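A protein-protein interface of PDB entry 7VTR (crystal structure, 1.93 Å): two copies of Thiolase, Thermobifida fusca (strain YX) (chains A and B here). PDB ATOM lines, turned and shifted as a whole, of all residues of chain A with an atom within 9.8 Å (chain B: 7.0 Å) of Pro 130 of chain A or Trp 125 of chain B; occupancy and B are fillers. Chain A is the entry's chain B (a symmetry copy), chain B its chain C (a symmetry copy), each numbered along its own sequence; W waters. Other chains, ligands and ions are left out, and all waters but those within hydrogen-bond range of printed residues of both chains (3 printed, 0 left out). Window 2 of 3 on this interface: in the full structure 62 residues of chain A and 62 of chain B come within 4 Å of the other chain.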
ATOM      1  N   ALA A  60      -2.579   8.934   7.257  1.00  0.00           N
ATOM      2  CA  ALA A  60      -3.056  10.216   6.745  1.00  0.00           C
ATOM      3  C   ALA A  60      -4.361  10.060   5.981  1.00  0.00           C
ATOM      4  O   ALA A  60      -5.138  11.015   5.895  1.00  0.00           O
ATOM      5  CB  ALA A  60      -2.002  10.861   5.847  1.00  0.00           C
ATOM      6  N   GLY A  61      -4.613   8.883   5.425  1.00  0.00           N
ATOM      7  CA  GLY A  61      -5.802   8.661   4.623  1.00  0.00           C
ATOM      8  C   GLY A  61      -7.012   8.202   5.393  1.00  0.00           C
ATOM      9  O   GLY A  61      -7.344   8.766   6.440  1.00  0.00           O
ATOM     10  N   PRO A 124      -2.915   8.553   0.696  1.00  0.00           N
ATOM     11  CA  PRO A 124      -3.331   9.789   0.034  1.00  0.00           C
ATOM     12  C   PRO A 124      -2.175  10.748  -0.196  1.00  0.00           C
ATOM     13  O   PRO A 124      -1.017  10.516   0.179  1.00  0.00           O
ATOM     14  CB  PRO A 124      -4.307  10.389   1.034  1.00  0.00           C
ATOM     15  CG  PRO A 124      -3.760   9.943   2.374  1.00  0.00           C
ATOM     16  CD  PRO A 124      -2.941   8.702   2.164  1.00  0.00           C
ATOM     17  N   TRP A 125      -2.531  11.871  -0.808  1.00  0.00           N
ATOM     18  CA  TRP A 125      -1.663  13.023  -0.835  1.00  0.00           C
ATOM     19  C   TRP A 125      -1.846  13.852   0.419  1.00  0.00           C
ATOM     20  O   TRP A 125      -2.938  13.920   0.995  1.00  0.00           O
ATOM     21  CB  TRP A 125      -1.962  13.907  -2.034  1.00  0.00           C
ATOM     22  CG  TRP A 125      -1.522  13.374  -3.325  1.00  0.00           C
ATOM     23  CD1 TRP A 125      -0.257  13.022  -3.701  1.00  0.00           C
ATOM     24  CD2 TRP A 125      -2.365  13.115  -4.440  1.00  0.00           C
ATOM     25  NE1 TRP A 125      -0.262  12.585  -5.010  1.00  0.00           N
ATOM     26  CE2 TRP A 125      -1.547  12.633  -5.481  1.00  0.00           C
ATOM     27  CE3 TRP A 125      -3.736  13.265  -4.667  1.00  0.00           C
ATOM     28  CZ2 TRP A 125      -2.060  12.301  -6.730  1.00  0.00           C
ATOM     29  CZ3 TRP A 125      -4.237  12.942  -5.914  1.00  0.00           C
ATOM     30  CH2 TRP A 125      -3.402  12.462  -6.923  1.00  0.00           C
ATOM     31  N   VAL A 126      -0.794  14.562   0.773  1.00  0.00           N
ATOM     32  CA  VAL A 126      -0.843  15.513   1.861  1.00  0.00           C
ATOM     33  C   VAL A 126      -0.385  16.837   1.293  1.00  0.00           C
ATOM     34  O   VAL A 126       0.633  16.899   0.592  1.00  0.00           O
ATOM     35  CB  VAL A 126       0.041  15.081   3.038  1.00  0.00           C
ATOM     36  CG1 VAL A 126       0.357  16.272   3.930  1.00  0.00           C
ATOM     37  CG2 VAL A 126      -0.623  13.921   3.791  1.00  0.00           C
ATOM     38  N   LEU A 127      -1.155  17.871   1.561  1.00  0.00           N
ATOM     39  CA  LEU A 127      -0.837  19.223   1.109  1.00  0.00           C
ATOM     40  C   LEU A 127      -0.645  20.108   2.328  1.00  0.00           C
ATOM     41  O   LEU A 127      -1.612  20.329   3.083  1.00  0.00           O
ATOM     42  CB  LEU A 127      -1.966  19.754   0.233  1.00  0.00           C
ATOM     43  CG  LEU A 127      -1.692  21.171  -0.264  1.00  0.00           C
ATOM     44  CD1 LEU A 127      -0.428  21.171  -1.096  1.00  0.00           C
ATOM     45  CD2 LEU A 127      -2.890  21.651  -1.075  1.00  0.00           C
ATOM     46  N   PRO A 128       0.562  20.600   2.591  1.00  0.00           N
ATOM     47  CA  PRO A 128       0.737  21.556   3.683  1.00  0.00           C
ATOM     48  C   PRO A 128      -0.094  22.802   3.450  1.00  0.00           C
ATOM     49  O   PRO A 128      -0.293  23.245   2.315  1.00  0.00           O
ATOM     50  CB  PRO A 128       2.237  21.871   3.639  1.00  0.00           C
ATOM     51  CG  PRO A 128       2.835  20.626   3.112  1.00  0.00           C
ATOM     52  CD  PRO A 128       1.864  20.202   2.023  1.00  0.00           C
ATOM     53  N   LYS A 129      -0.595  23.339   4.531  1.00  0.00           N
ATOM     54  CA  LYS A 129      -1.314  24.598   4.514  1.00  0.00           C
ATOM     55  C   LYS A 129      -0.334  25.763   4.525  1.00  0.00           C
ATOM     56  O   LYS A 129       0.717  25.690   5.175  1.00  0.00           O
ATOM     57  CB  LYS A 129      -2.221  24.691   5.728  1.00  0.00           C
ATOM     58  CG  LYS A 129      -3.226  23.606   5.713  1.00  0.00           C
ATOM     59  CD  LYS A 129      -4.412  23.964   6.522  1.00  0.00           C
ATOM     60  CE  LYS A 129      -5.385  22.814   6.558  1.00  0.00           C
ATOM     61  NZ  LYS A 129      -5.964  22.772   7.900  1.00  0.00           N
ATOM     62  N   PRO A 130      -0.659  26.854   3.820  1.00  0.00           N
ATOM     63  CA  PRO A 130       0.177  28.057   3.908  1.00  0.00           C
ATOM     64  C   PRO A 130       0.022  28.711   5.265  1.00  0.00           C
ATOM     65  O   PRO A 130      -1.071  28.739   5.832  1.00  0.00           O
ATOM     66  CB  PRO A 130      -0.383  28.962   2.810  1.00  0.00           C
ATOM     67  CG  PRO A 130      -1.833  28.571   2.749  1.00  0.00           C
ATOM     68  CD  PRO A 130      -1.823  27.060   2.937  1.00  0.00           C
ATOM     69  N   ALA A 131       1.138  29.234   5.782  1.00  0.00           N
ATOM     70  CA  ALA A 131       1.112  30.015   7.014  1.00  0.00           C
ATOM     71  C   ALA A 131       0.506  31.389   6.808  1.00  0.00           C
ATOM     72  O   ALA A 131       0.081  32.025   7.776  1.00  0.00           O
ATOM     73  CB  ALA A 131       2.522  30.178   7.565  1.00  0.00           C
ATOM     74  N   GLN A 132       0.464  31.868   5.574  1.00  0.00           N
ATOM     75  CA  GLN A 132      -0.054  33.194   5.291  1.00  0.00           C
ATOM     76  C   GLN A 132      -1.067  33.070   4.169  1.00  0.00           C
ATOM     77  O   GLN A 132      -1.062  32.097   3.413  1.00  0.00           O
ATOM     78  CB  GLN A 132       1.068  34.135   4.895  1.00  0.00           C
ATOM     79  CG  GLN A 132       1.727  34.793   6.090  1.00  0.00           C
ATOM     80  CD  GLN A 132       3.041  35.410   5.710  1.00  0.00           C
ATOM     81  OE1 GLN A 132       3.389  36.497   6.174  1.00  0.00           O
ATOM     82  NE2 GLN A 132       3.787  34.718   4.848  1.00  0.00           N
ATOM     83  N   GLY A 133      -1.947  34.053   4.077  1.00  0.00           N
ATOM     84  CA  GLY A 133      -2.917  34.050   3.016  1.00  0.00           C
ATOM     85  C   GLY A 133      -2.263  34.244   1.667  1.00  0.00           C
ATOM     86  O   GLY A 133      -1.120  34.685   1.558  1.00  0.00           O
ATOM     87  N   PHE A 134      -3.006  33.893   0.623  1.00  0.00           N
ATOM     88  CA  PHE A 134      -2.575  34.032  -0.766  1.00  0.00           C
ATOM     89  C   PHE A 134      -1.099  33.656  -0.934  1.00  0.00           C
ATOM     90  O   PHE A 134      -0.283  34.501  -1.317  1.00  0.00           O
ATOM     91  CB  PHE A 134      -2.830  35.446  -1.266  1.00  0.00           C
ATOM     92  CG  PHE A 134      -4.217  35.930  -0.997  1.00  0.00           C
ATOM     93  CD1 PHE A 134      -5.306  35.331  -1.594  1.00  0.00           C
ATOM     94  CD2 PHE A 134      -4.423  36.949  -0.094  1.00  0.00           C
ATOM     95  CE1 PHE A 134      -6.588  35.780  -1.339  1.00  0.00           C
ATOM     96  CE2 PHE A 134      -5.687  37.392   0.191  1.00  0.00           C
ATOM     97  CZ  PHE A 134      -6.772  36.828  -0.439  1.00  0.00           C
ATOM     98  N   PRO A 135      -0.726  32.419  -0.632  1.00  0.00           N
ATOM     99  CA  PRO A 135       0.623  31.981  -0.980  1.00  0.00           C
ATOM    100  C   PRO A 135       0.811  32.165  -2.467  1.00  0.00           C
ATOM    101  O   PRO A 135      -0.113  31.962  -3.258  1.00  0.00           O
ATOM    102  CB  PRO A 135       0.633  30.498  -0.603  1.00  0.00           C
ATOM    103  CG  PRO A 135      -0.795  30.137  -0.460  1.00  0.00           C
ATOM    104  CD  PRO A 135      -1.501  31.348   0.008  1.00  0.00           C
ATOM    105  N   THR A 136       1.975  32.592  -2.882  1.00  0.00           N
ATOM    106  CA  THR A 136       2.159  32.790  -4.291  1.00  0.00           C
ATOM    107  C   THR A 136       2.781  31.650  -5.024  1.00  0.00           C
ATOM    108  O   THR A 136       2.514  31.472  -6.186  1.00  0.00           O
ATOM    109  CB  THR A 136       3.063  33.983  -4.580  1.00  0.00           C
ATOM    110  OG1 THR A 136       4.358  33.713  -4.052  1.00  0.00           O
ATOM    111  CG2 THR A 136       2.496  35.228  -3.980  1.00  0.00           C
ATOM    112  N   GLY A 137       3.643  30.912  -4.359  1.00  0.00           N
ATOM    113  CA  GLY A 137       4.363  29.847  -5.011  1.00  0.00           C
ATOM    114  C   GLY A 137       3.767  28.473  -5.167  1.00  0.00           C
ATOM    115  O   GLY A 137       2.788  28.143  -4.560  1.00  0.00           O
ATOM    116  N   HIS A 138       4.404  27.700  -6.025  1.00  0.00           N
ATOM    117  CA  HIS A 138       4.045  26.329  -6.279  1.00  0.00           C
ATOM    118  C   HIS A 138       4.369  25.546  -5.013  1.00  0.00           C
ATOM    119  O   HIS A 138       5.423  25.750  -4.421  1.00  0.00           O
ATOM    120  CB  HIS A 138       4.931  25.722  -7.370  1.00  0.00           C
ATOM    121  CG  HIS A 138       4.807  26.354  -8.717  1.00  0.00           C
ATOM    122  ND1 HIS A 138       3.688  27.030  -9.135  1.00  0.00           N
ATOM    123  CD2 HIS A 138       5.661  26.361  -9.763  1.00  0.00           C
ATOM    124  CE1 HIS A 138       3.868  27.450 -10.368  1.00  0.00           C
ATOM    125  NE2 HIS A 138       5.059  27.060 -10.774  1.00  0.00           N
ATOM    126  N   GLU A 139       3.481  24.651  -4.621  1.00  0.00           N
ATOM    127  CA  GLU A 139       3.644  23.743  -3.502  1.00  0.00           C
ATOM    128  C   GLU A 139       3.762  22.308  -3.982  1.00  0.00           C
ATOM    129  O   GLU A 139       3.383  21.962  -5.102  1.00  0.00           O
ATOM    130  CB  GLU A 139       2.494  23.853  -2.490  1.00  0.00           C
ATOM    131  CG  GLU A 139       1.800  25.221  -2.253  1.00  0.00           C
ATOM    132  CD  GLU A 139       2.739  26.421  -2.052  1.00  0.00           C
ATOM    133  OE1 GLU A 139       3.977  26.266  -2.177  1.00  0.00           O
ATOM    134  OE2 GLU A 139       2.234  27.527  -1.721  1.00  0.00           O
ATOM    135  N   THR A 140       4.318  21.485  -3.115  1.00  0.00           N
ATOM    136  CA  THR A 140       4.380  20.064  -3.353  1.00  0.00           C
ATOM    137  C   THR A 140       3.183  19.383  -2.717  1.00  0.00           C
ATOM    138  O   THR A 140       2.895  19.570  -1.532  1.00  0.00           O
ATOM    139  CB  THR A 140       5.689  19.500  -2.822  1.00  0.00           C
ATOM    140  OG1 THR A 140       6.771  20.236  -3.404  1.00  0.00           O
ATOM    141  CG2 THR A 140       5.810  18.022  -3.161  1.00  0.00           C
ATOM    142  N   LEU A 141       2.479  18.612  -3.520  1.00  0.00           N
ATOM    143  CA  LEU A 141       1.466  17.701  -3.038  1.00  0.00           C
ATOM    144  C   LEU A 141       2.186  16.392  -2.744  1.00  0.00           C
ATOM    145  O   LEU A 141       2.595  15.689  -3.666  1.00  0.00           O
ATOM    146  CB  LEU A 141       0.388  17.526  -4.096  1.00  0.00           C
ATOM    147  CG  LEU A 141      -0.813  16.700  -3.675  1.00  0.00           C
ATOM    148  CD1 LEU A 141      -1.546  17.383  -2.544  1.00  0.00           C
ATOM    149  CD2 LEU A 141      -1.727  16.395  -4.867  1.00  0.00           C
ATOM    150  N   TYR A 142       2.388  16.086  -1.470  1.00  0.00           N
ATOM    151  CA  TYR A 142       3.210  14.944  -1.098  1.00  0.00           C
ATOM    152  C   TYR A 142       2.384  13.676  -1.184  1.00  0.00           C
ATOM    153  O   TYR A 142       1.290  13.604  -0.621  1.00  0.00           O
ATOM    154  CB  TYR A 142       3.765  15.124   0.311  1.00  0.00           C
ATOM    155  CG  TYR A 142       4.739  16.269   0.381  1.00  0.00           C
ATOM    156  CD1 TYR A 142       6.069  16.114  -0.002  1.00  0.00           C
ATOM    157  CD2 TYR A 142       4.301  17.528   0.745  1.00  0.00           C
ATOM    158  CE1 TYR A 142       6.956  17.206   0.040  1.00  0.00           C
ATOM    159  CE2 TYR A 142       5.159  18.594   0.796  1.00  0.00           C
ATOM    160  CZ  TYR A 142       6.474  18.435   0.439  1.00  0.00           C
ATOM    161  OH  TYR A 142       7.274  19.546   0.520  1.00  0.00           O
ATOM    162  N   SER A 143       2.903  12.686  -1.888  1.00  0.00           N
ATOM    163  CA  SER A 143       2.316  11.368  -1.825  1.00  0.00           C
ATOM    164  C   SER A 143       2.836  10.696  -0.564  1.00  0.00           C
ATOM    165  O   SER A 143       4.028  10.786  -0.258  1.00  0.00           O
ATOM    166  CB  SER A 143       2.675  10.544  -3.058  1.00  0.00           C
ATOM    167  OG  SER A 143       2.223   9.217  -2.899  1.00  0.00           O
ATOM    168  N   THR A 144       1.935  10.093   0.192  1.00  0.00           N
ATOM    169  CA  THR A 144       2.311   9.370   1.394  1.00  0.00           C
ATOM    170  C   THR A 144       2.621   7.923   1.097  1.00  0.00           C
ATOM    171  O   THR A 144       2.832   7.143   2.029  1.00  0.00           O
ATOM    172  CB  THR A 144       1.201   9.449   2.448  1.00  0.00           C
ATOM    173  OG1 THR A 144       0.034   8.782   1.969  1.00  0.00           O
ATOM    174  CG2 THR A 144       0.868  10.888   2.779  1.00  0.00           C
ATOM    175  N   ARG A 149       8.794  12.738   2.902  1.00  0.00           N
ATOM    176  CA  ARG A 149       7.921  13.788   2.424  1.00  0.00           C
ATOM    177  C   ARG A 149       7.940  14.879   3.466  1.00  0.00           C
ATOM    178  O   ARG A 149       8.078  14.597   4.662  1.00  0.00           O
ATOM    179  CB  ARG A 149       6.507  13.266   2.215  1.00  0.00           C
ATOM    180  CG  ARG A 149       5.997  12.423   3.394  1.00  0.00           C
ATOM    181  CD  ARG A 149       4.533  12.050   3.152  1.00  0.00           C
ATOM    182  NE  ARG A 149       4.011  11.077   4.105  1.00  0.00           N
ATOM    183  CZ  ARG A 149       4.381   9.804   4.178  1.00  0.00           C
ATOM    184  NH1 ARG A 149       5.253   9.287   3.329  1.00  0.00           N
ATOM    185  NH2 ARG A 149       3.832   9.023   5.106  1.00  0.00           N
ATOM    186  N   MET A 150       7.781  16.120   3.022  1.00  0.00           N
ATOM    187  CA  MET A 150       7.816  17.223   3.964  1.00  0.00           C
ATOM    188  C   MET A 150       9.090  17.114   4.800  1.00  0.00           C
ATOM    189  O   MET A 150       9.056  17.157   6.032  1.00  0.00           O
ATOM    190  CB  MET A 150       6.565  17.234   4.852  1.00  0.00           C
ATOM    191  CG  MET A 150       5.358  17.910   4.268  1.00  0.00           C
ATOM    192  SD  MET A 150       3.745  17.307   4.806  1.00  0.00           S
ATOM    193  CE  MET A 150       3.873  15.526   4.692  1.00  0.00           C
ATOM    194  N   ALA B  60       0.071  13.633   9.780  1.00  0.00           N
ATOM    195  CA  ALA B  60       0.038  13.702   8.333  1.00  0.00           C
ATOM    196  C   ALA B  60       0.969  14.779   7.803  1.00  0.00           C
ATOM    197  O   ALA B  60       1.409  14.691   6.651  1.00  0.00           O
ATOM    198  CB  ALA B  60      -1.396  13.957   7.859  1.00  0.00           C
ATOM    199  N   SER B 121      -1.988  24.065  14.154  1.00  0.00           N
ATOM    200  CA  SER B 121      -1.840  25.081  13.109  1.00  0.00           C
ATOM    201  C   SER B 121      -1.457  24.451  11.782  1.00  0.00           C
ATOM    202  O   SER B 121      -2.117  24.665  10.758  1.00  0.00           O
ATOM    203  CB  SER B 121      -0.773  26.089  13.508  1.00  0.00           C
ATOM    204  OG  SER B 121      -1.160  26.787  14.672  1.00  0.00           O
ATOM    205  N   ARG B 122      -0.373  23.681  11.780  1.00  0.00           N
ATOM    206  CA  ARG B 122       0.216  23.181  10.557  1.00  0.00           C
ATOM    207  C   ARG B 122      -0.344  21.833  10.148  1.00  0.00           C
ATOM    208  O   ARG B 122       0.265  21.156   9.319  1.00  0.00           O
ATOM    209  CB  ARG B 122       1.742  23.131  10.691  1.00  0.00           C
ATOM    210  CG  ARG B 122       2.327  24.384  11.336  1.00  0.00           C
ATOM    211  CD  ARG B 122       3.824  24.250  11.508  1.00  0.00           C
ATOM    212  NE  ARG B 122       4.490  24.136  10.212  1.00  0.00           N
ATOM    213  CZ  ARG B 122       4.942  25.163   9.502  1.00  0.00           C
ATOM    214  NH1 ARG B 122       4.711  26.415   9.876  1.00  0.00           N
ATOM    215  NH2 ARG B 122       5.631  24.926   8.391  1.00  0.00           N
ATOM    216  N   ALA B 123      -1.482  21.437  10.718  1.00  0.00           N
ATOM    217  CA  ALA B 123      -2.225  20.254  10.329  1.00  0.00           C
ATOM    218  C   ALA B 123      -2.501  20.366   8.844  1.00  0.00           C
ATOM    219  O   ALA B 123      -3.254  21.254   8.430  1.00  0.00           O
ATOM    220  CB  ALA B 123      -3.536  20.156  11.107  1.00  0.00           C
ATOM    221  N   PRO B 124      -1.922  19.514   8.012  1.00  0.00           N
ATOM    222  CA  PRO B 124      -2.069  19.727   6.571  1.00  0.00           C
ATOM    223  C   PRO B 124      -3.425  19.330   6.049  1.00  0.00           C
ATOM    224  O   PRO B 124      -4.316  18.888   6.784  1.00  0.00           O
ATOM    225  CB  PRO B 124      -0.968  18.849   5.977  1.00  0.00           C
ATOM    226  CG  PRO B 124      -0.913  17.690   6.924  1.00  0.00           C
ATOM    227  CD  PRO B 124      -1.236  18.242   8.311  1.00  0.00           C
ATOM    228  N   TRP B 125      -3.575  19.513   4.748  1.00  0.00           N
ATOM    229  CA  TRP B 125      -4.681  18.957   4.003  1.00  0.00           C
ATOM    230  C   TRP B 125      -4.326  17.560   3.539  1.00  0.00           C
ATOM    231  O   TRP B 125      -3.160  17.229   3.344  1.00  0.00           O
ATOM    232  CB  TRP B 125      -4.972  19.808   2.780  1.00  0.00           C
ATOM    233  CG  TRP B 125      -5.684  21.074   3.016  1.00  0.00           C
ATOM    234  CD1 TRP B 125      -6.900  21.252   3.609  1.00  0.00           C
ATOM    235  CD2 TRP B 125      -5.228  22.372   2.626  1.00  0.00           C
ATOM    236  NE1 TRP B 125      -7.226  22.593   3.614  1.00  0.00           N
ATOM    237  CE2 TRP B 125      -6.221  23.297   3.002  1.00  0.00           C
ATOM    238  CE3 TRP B 125      -4.076  22.840   1.985  1.00  0.00           C
ATOM    239  CZ2 TRP B 125      -6.098  24.657   2.753  1.00  0.00           C
ATOM    240  CZ3 TRP B 125      -3.950  24.197   1.742  1.00  0.00           C
ATOM    241  CH2 TRP B 125      -4.950  25.090   2.125  1.00  0.00           C
ATOM    242  N   VAL B 126      -5.344  16.748   3.352  1.00  0.00           N
ATOM    243  CA  VAL B 126      -5.173  15.410   2.820  1.00  0.00           C
ATOM    244  C   VAL B 126      -6.101  15.275   1.632  1.00  0.00           C
ATOM    245  O   VAL B 126      -7.292  15.605   1.726  1.00  0.00           O
ATOM    246  CB  VAL B 126      -5.468  14.323   3.857  1.00  0.00           C
ATOM    247  CG1 VAL B 126      -5.546  12.957   3.161  1.00  0.00           C
ATOM    248  CG2 VAL B 126      -4.397  14.316   4.904  1.00  0.00           C
ATOM    249  N   LEU B 127      -5.548  14.830   0.522  1.00  0.00           N
ATOM    250  CA  LEU B 127      -6.318  14.589  -0.695  1.00  0.00           C
ATOM    251  C   LEU B 127      -6.236  13.118  -1.056  1.00  0.00           C
ATOM    252  O   LEU B 127      -5.143  12.631  -1.406  1.00  0.00           O
ATOM    253  CB  LEU B 127      -5.804  15.465  -1.836  1.00  0.00           C
ATOM    254  CG  LEU B 127      -6.582  15.284  -3.147  1.00  0.00           C
ATOM    255  CD1 LEU B 127      -8.047  15.688  -2.989  1.00  0.00           C
ATOM    256  CD2 LEU B 127      -5.893  16.133  -4.206  1.00  0.00           C
ATOM    257  N   LEU B 141     -10.803  18.286  -0.388  1.00  0.00           N
ATOM    258  CA  LEU B 141      -9.493  18.376   0.223  1.00  0.00           C
ATOM    259  C   LEU B 141      -9.759  18.414   1.726  1.00  0.00           C
ATOM    260  O   LEU B 141     -10.305  19.401   2.240  1.00  0.00           O
ATOM    261  CB  LEU B 141      -8.776  19.637  -0.231  1.00  0.00           C
ATOM    262  CG  LEU B 141      -7.319  19.761   0.159  1.00  0.00           C
ATOM    263  CD1 LEU B 141      -6.483  18.618  -0.417  1.00  0.00           C
ATOM    264  CD2 LEU B 141      -6.772  21.148  -0.160  1.00  0.00           C
ATOM    265  N   TYR B 142      -9.434  17.331   2.424  1.00  0.00           N
ATOM    266  CA  TYR B 142      -9.712  17.273   3.853  1.00  0.00           C
ATOM    267  C   TYR B 142      -8.657  17.999   4.650  1.00  0.00           C
ATOM    268  O   TYR B 142      -7.465  17.733   4.505  1.00  0.00           O
ATOM    269  CB  TYR B 142      -9.811  15.839   4.354  1.00  0.00           C
ATOM    270  CG  TYR B 142     -10.831  15.068   3.604  1.00  0.00           C
ATOM    271  CD1 TYR B 142     -10.524  14.468   2.391  1.00  0.00           C
ATOM    272  CD2 TYR B 142     -12.138  14.982   4.079  1.00  0.00           C
ATOM    273  CE1 TYR B 142     -11.466  13.762   1.705  1.00  0.00           C
ATOM    274  CE2 TYR B 142     -13.093  14.280   3.381  1.00  0.00           C
ATOM    275  CZ  TYR B 142     -12.752  13.685   2.198  1.00  0.00           C
ATOM    276  OH  TYR B 142     -13.701  13.000   1.492  1.00  0.00           O
ATOM    277  N   SER B 143      -9.116  18.889   5.512  1.00  0.00           N
ATOM    278  CA  SER B 143      -8.286  19.464   6.540  1.00  0.00           C
ATOM    279  C   SER B 143      -8.109  18.473   7.678  1.00  0.00           C
ATOM    280  O   SER B 143      -9.068  17.841   8.125  1.00  0.00           O
ATOM    281  CB  SER B 143      -8.942  20.731   7.068  1.00  0.00           C
ATOM    282  OG  SER B 143      -8.147  21.248   8.097  1.00  0.00           O
ATOM    283  N   THR B 144      -6.875  18.340   8.159  1.00  0.00           N
ATOM    284  CA  THR B 144      -6.596  17.455   9.282  1.00  0.00           C
ATOM    285  C   THR B 144      -6.609  18.198  10.599  1.00  0.00           C
ATOM    286  O   THR B 144      -6.147  17.672  11.613  1.00  0.00           O
ATOM    287  CB  THR B 144      -5.259  16.744   9.095  1.00  0.00           C
ATOM    288  OG1 THR B 144      -4.212  17.715   9.045  1.00  0.00           O
ATOM    289  CG2 THR B 144      -5.268  15.931   7.834  1.00  0.00           C
ATOM    290  N   THR B 145      -7.140  19.411  10.603  1.00  0.00           N
ATOM    291  CA  THR B 145      -7.050  20.241  11.787  1.00  0.00           C
ATOM    292  C   THR B 145      -7.977  19.738  12.875  1.00  0.00           C
ATOM    293  O   THR B 145      -7.587  19.649  14.042  1.00  0.00           O
ATOM    294  CB  THR B 145      -7.400  21.676  11.422  1.00  0.00           C
ATOM    295  OG1 THR B 145      -6.545  22.082  10.353  1.00  0.00           O
ATOM    296  CG2 THR B 145      -7.142  22.570  12.614  1.00  0.00           C
HETATM  297  O   HOH W   1       2.160  12.369   5.598  1.00  0.00           O
HETATM  298  O   HOH W   2      -4.521  23.450  10.103  1.00  0.00           O
HETATM  299  O   HOH W   3       0.610  22.384   6.998  1.00  0.00           O
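The backbone carbonyl oxygen (O) of Leu 127 of chain B sits at hydrogen-bond distance from the backbone NH (N) of Trp 125 of chain A (2.8 Å).
The backbone carbonyl oxygen (O) of Leu 127 of chain A is in hydrogen-bond range of the backbone NH (N) of Trp 125 of chain B, 2.7 Å away.
The side-chain amino group (NZ) of Lys 129 of chain A sits at hydrogen-bond distance from the backbone carbonyl oxygen (O) of Ala 123 of chain B (3.2 Å).
The side-chain hydroxyl (OG) of Ser 143 of chain B sits at hydrogen-bond distance from the side-chain amino group (NZ) of Lys 129 of chain A (2.7 Å).
The side-chain amino group (NZ) of Lys 129 of chain A lies within hydrogen-bond range of the side-chain hydroxyl (OG1) of Thr 145 of chain B (2.6 Å).
OG1 of Thr 144 of chain A is in hydrogen-bond range of O of Pro 124 of chain A (2.7 Å).
The side-chain hydroxyl (OG1) of Thr 144 of chain B lies within hydrogen-bond range of the backbone carbonyl oxygen (O) of Pro 124 of chain B, 2.5 Å away.
The backbone NH of Val 126 of chain B is in hydrogen-bond range of the backbone carbonyl oxygen of Tyr 142 of chain B, 2.6 Å away.
Val 126 of chain B touches Ala 60 of chain A.
Val 126 of chain B touches Trp 125 of chain A.
CG1 of Val 126 of chain A touches O of Ala 60 of chain B, at 3.3 Å.
Trp 125 of chain B touches Val 126 of chain A (O to CA, 3.2 Å).
Val 126 of chain A touches Val 126 of chain B.
Pro 124 of chain B touches Leu 127 of chain A (CB to O, 3.3 Å).
Pro 128 of chain A touches Pro 124 of chain B.
Trp 125 of chain B touches Lys 129 of chain A (NE1 to CE, 3.5 Å).
Printed residues of chain B within 4 Å of Val 126 of chain A: Ala 60 (3.3 Å), Pro 124 (3.5 Å), Trp 125 (3.2 Å) and Val 126 (3.95 Å).
Printed residues of chain B within 4 Å of Leu 127 of chain A: Pro 124 and Trp 125.
Pro 130 of chain A touches just one residue of chain B: Trp 125 (3.8 Å).
Phe 134 of chain A touches none of the printed residues of chain B.
Printed residues of chain B within 4 Å of Met 150 of chain A: Ala 60 (3.3 Å).
Of chain A, only Val 126, Leu 127 and Pro 128 come within 4 Å of Pro 124 of chain B.
Trp 125 of chain B touches just these residues of chain A: Val 126 (3.2 Å), Leu 127 (2.7 Å), Pro 128 (3.8 Å), Lys 129 (3.5 Å) and Pro 130 (3.8 Å).
Leu 141 of chain B touches none of the printed residues of chain A.
The nearest residue of chain A that does not touch Trp 125 of chain B is Trp 125 of chain A (4.1 Å).
Printed residues of chain B that touch a printed residue of chain A: Ala 60, Ala 123, Pro 124, Trp 125, Val 126, Leu 127, Ser 143 and Thr 145.
Hydrophobic or aromatic side chains of chain B within 4 Å of the printed part of chain A: Ala 60, Pro 124, Trp 125, Val 126 and Leu 127.
Of the 25 printed residues of chain A, 9 touch a printed residue of chain B.
Hydrophobic or aromatic side chains of chain A that line the printed part of chain B: Ala 60, Pro 124, Trp 125, Val 126, Leu 127, Pro 130 and Met 150.
Among the printed residues, no Asp or Glu carboxylate lies within 4 Å of a Lys or Arg side-chain nitrogen of the other chain.
Ala 60 of chain B touches its own counterpart, Ala 60 of chain A.
Pro 124 of chain A touches Val 126 of chain B, and with the chains exchanged Val 126 of chain A touches Pro 124 of chain B.
Val 126 of chain B touches its own counterpart, Val 126 of chain A.
Of the 20 pairs that touch across the chains among the printed residues, 12 have their exchanged pair printed and touching as well.
Water W2 lies within hydrogen-bond range of OG1 of Thr 145 of chain B, NZ of Lys 129 of chain A, O of Ser 121 of chain B and O of Ala 123 of chain B.
Water W3 lies within hydrogen-bond range of the backbone carbonyl oxygen (O) of Arg 122 of chain B (2.6 Å) and the backbone NH (N) of Lys 129 of chain A (2.9 Å).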
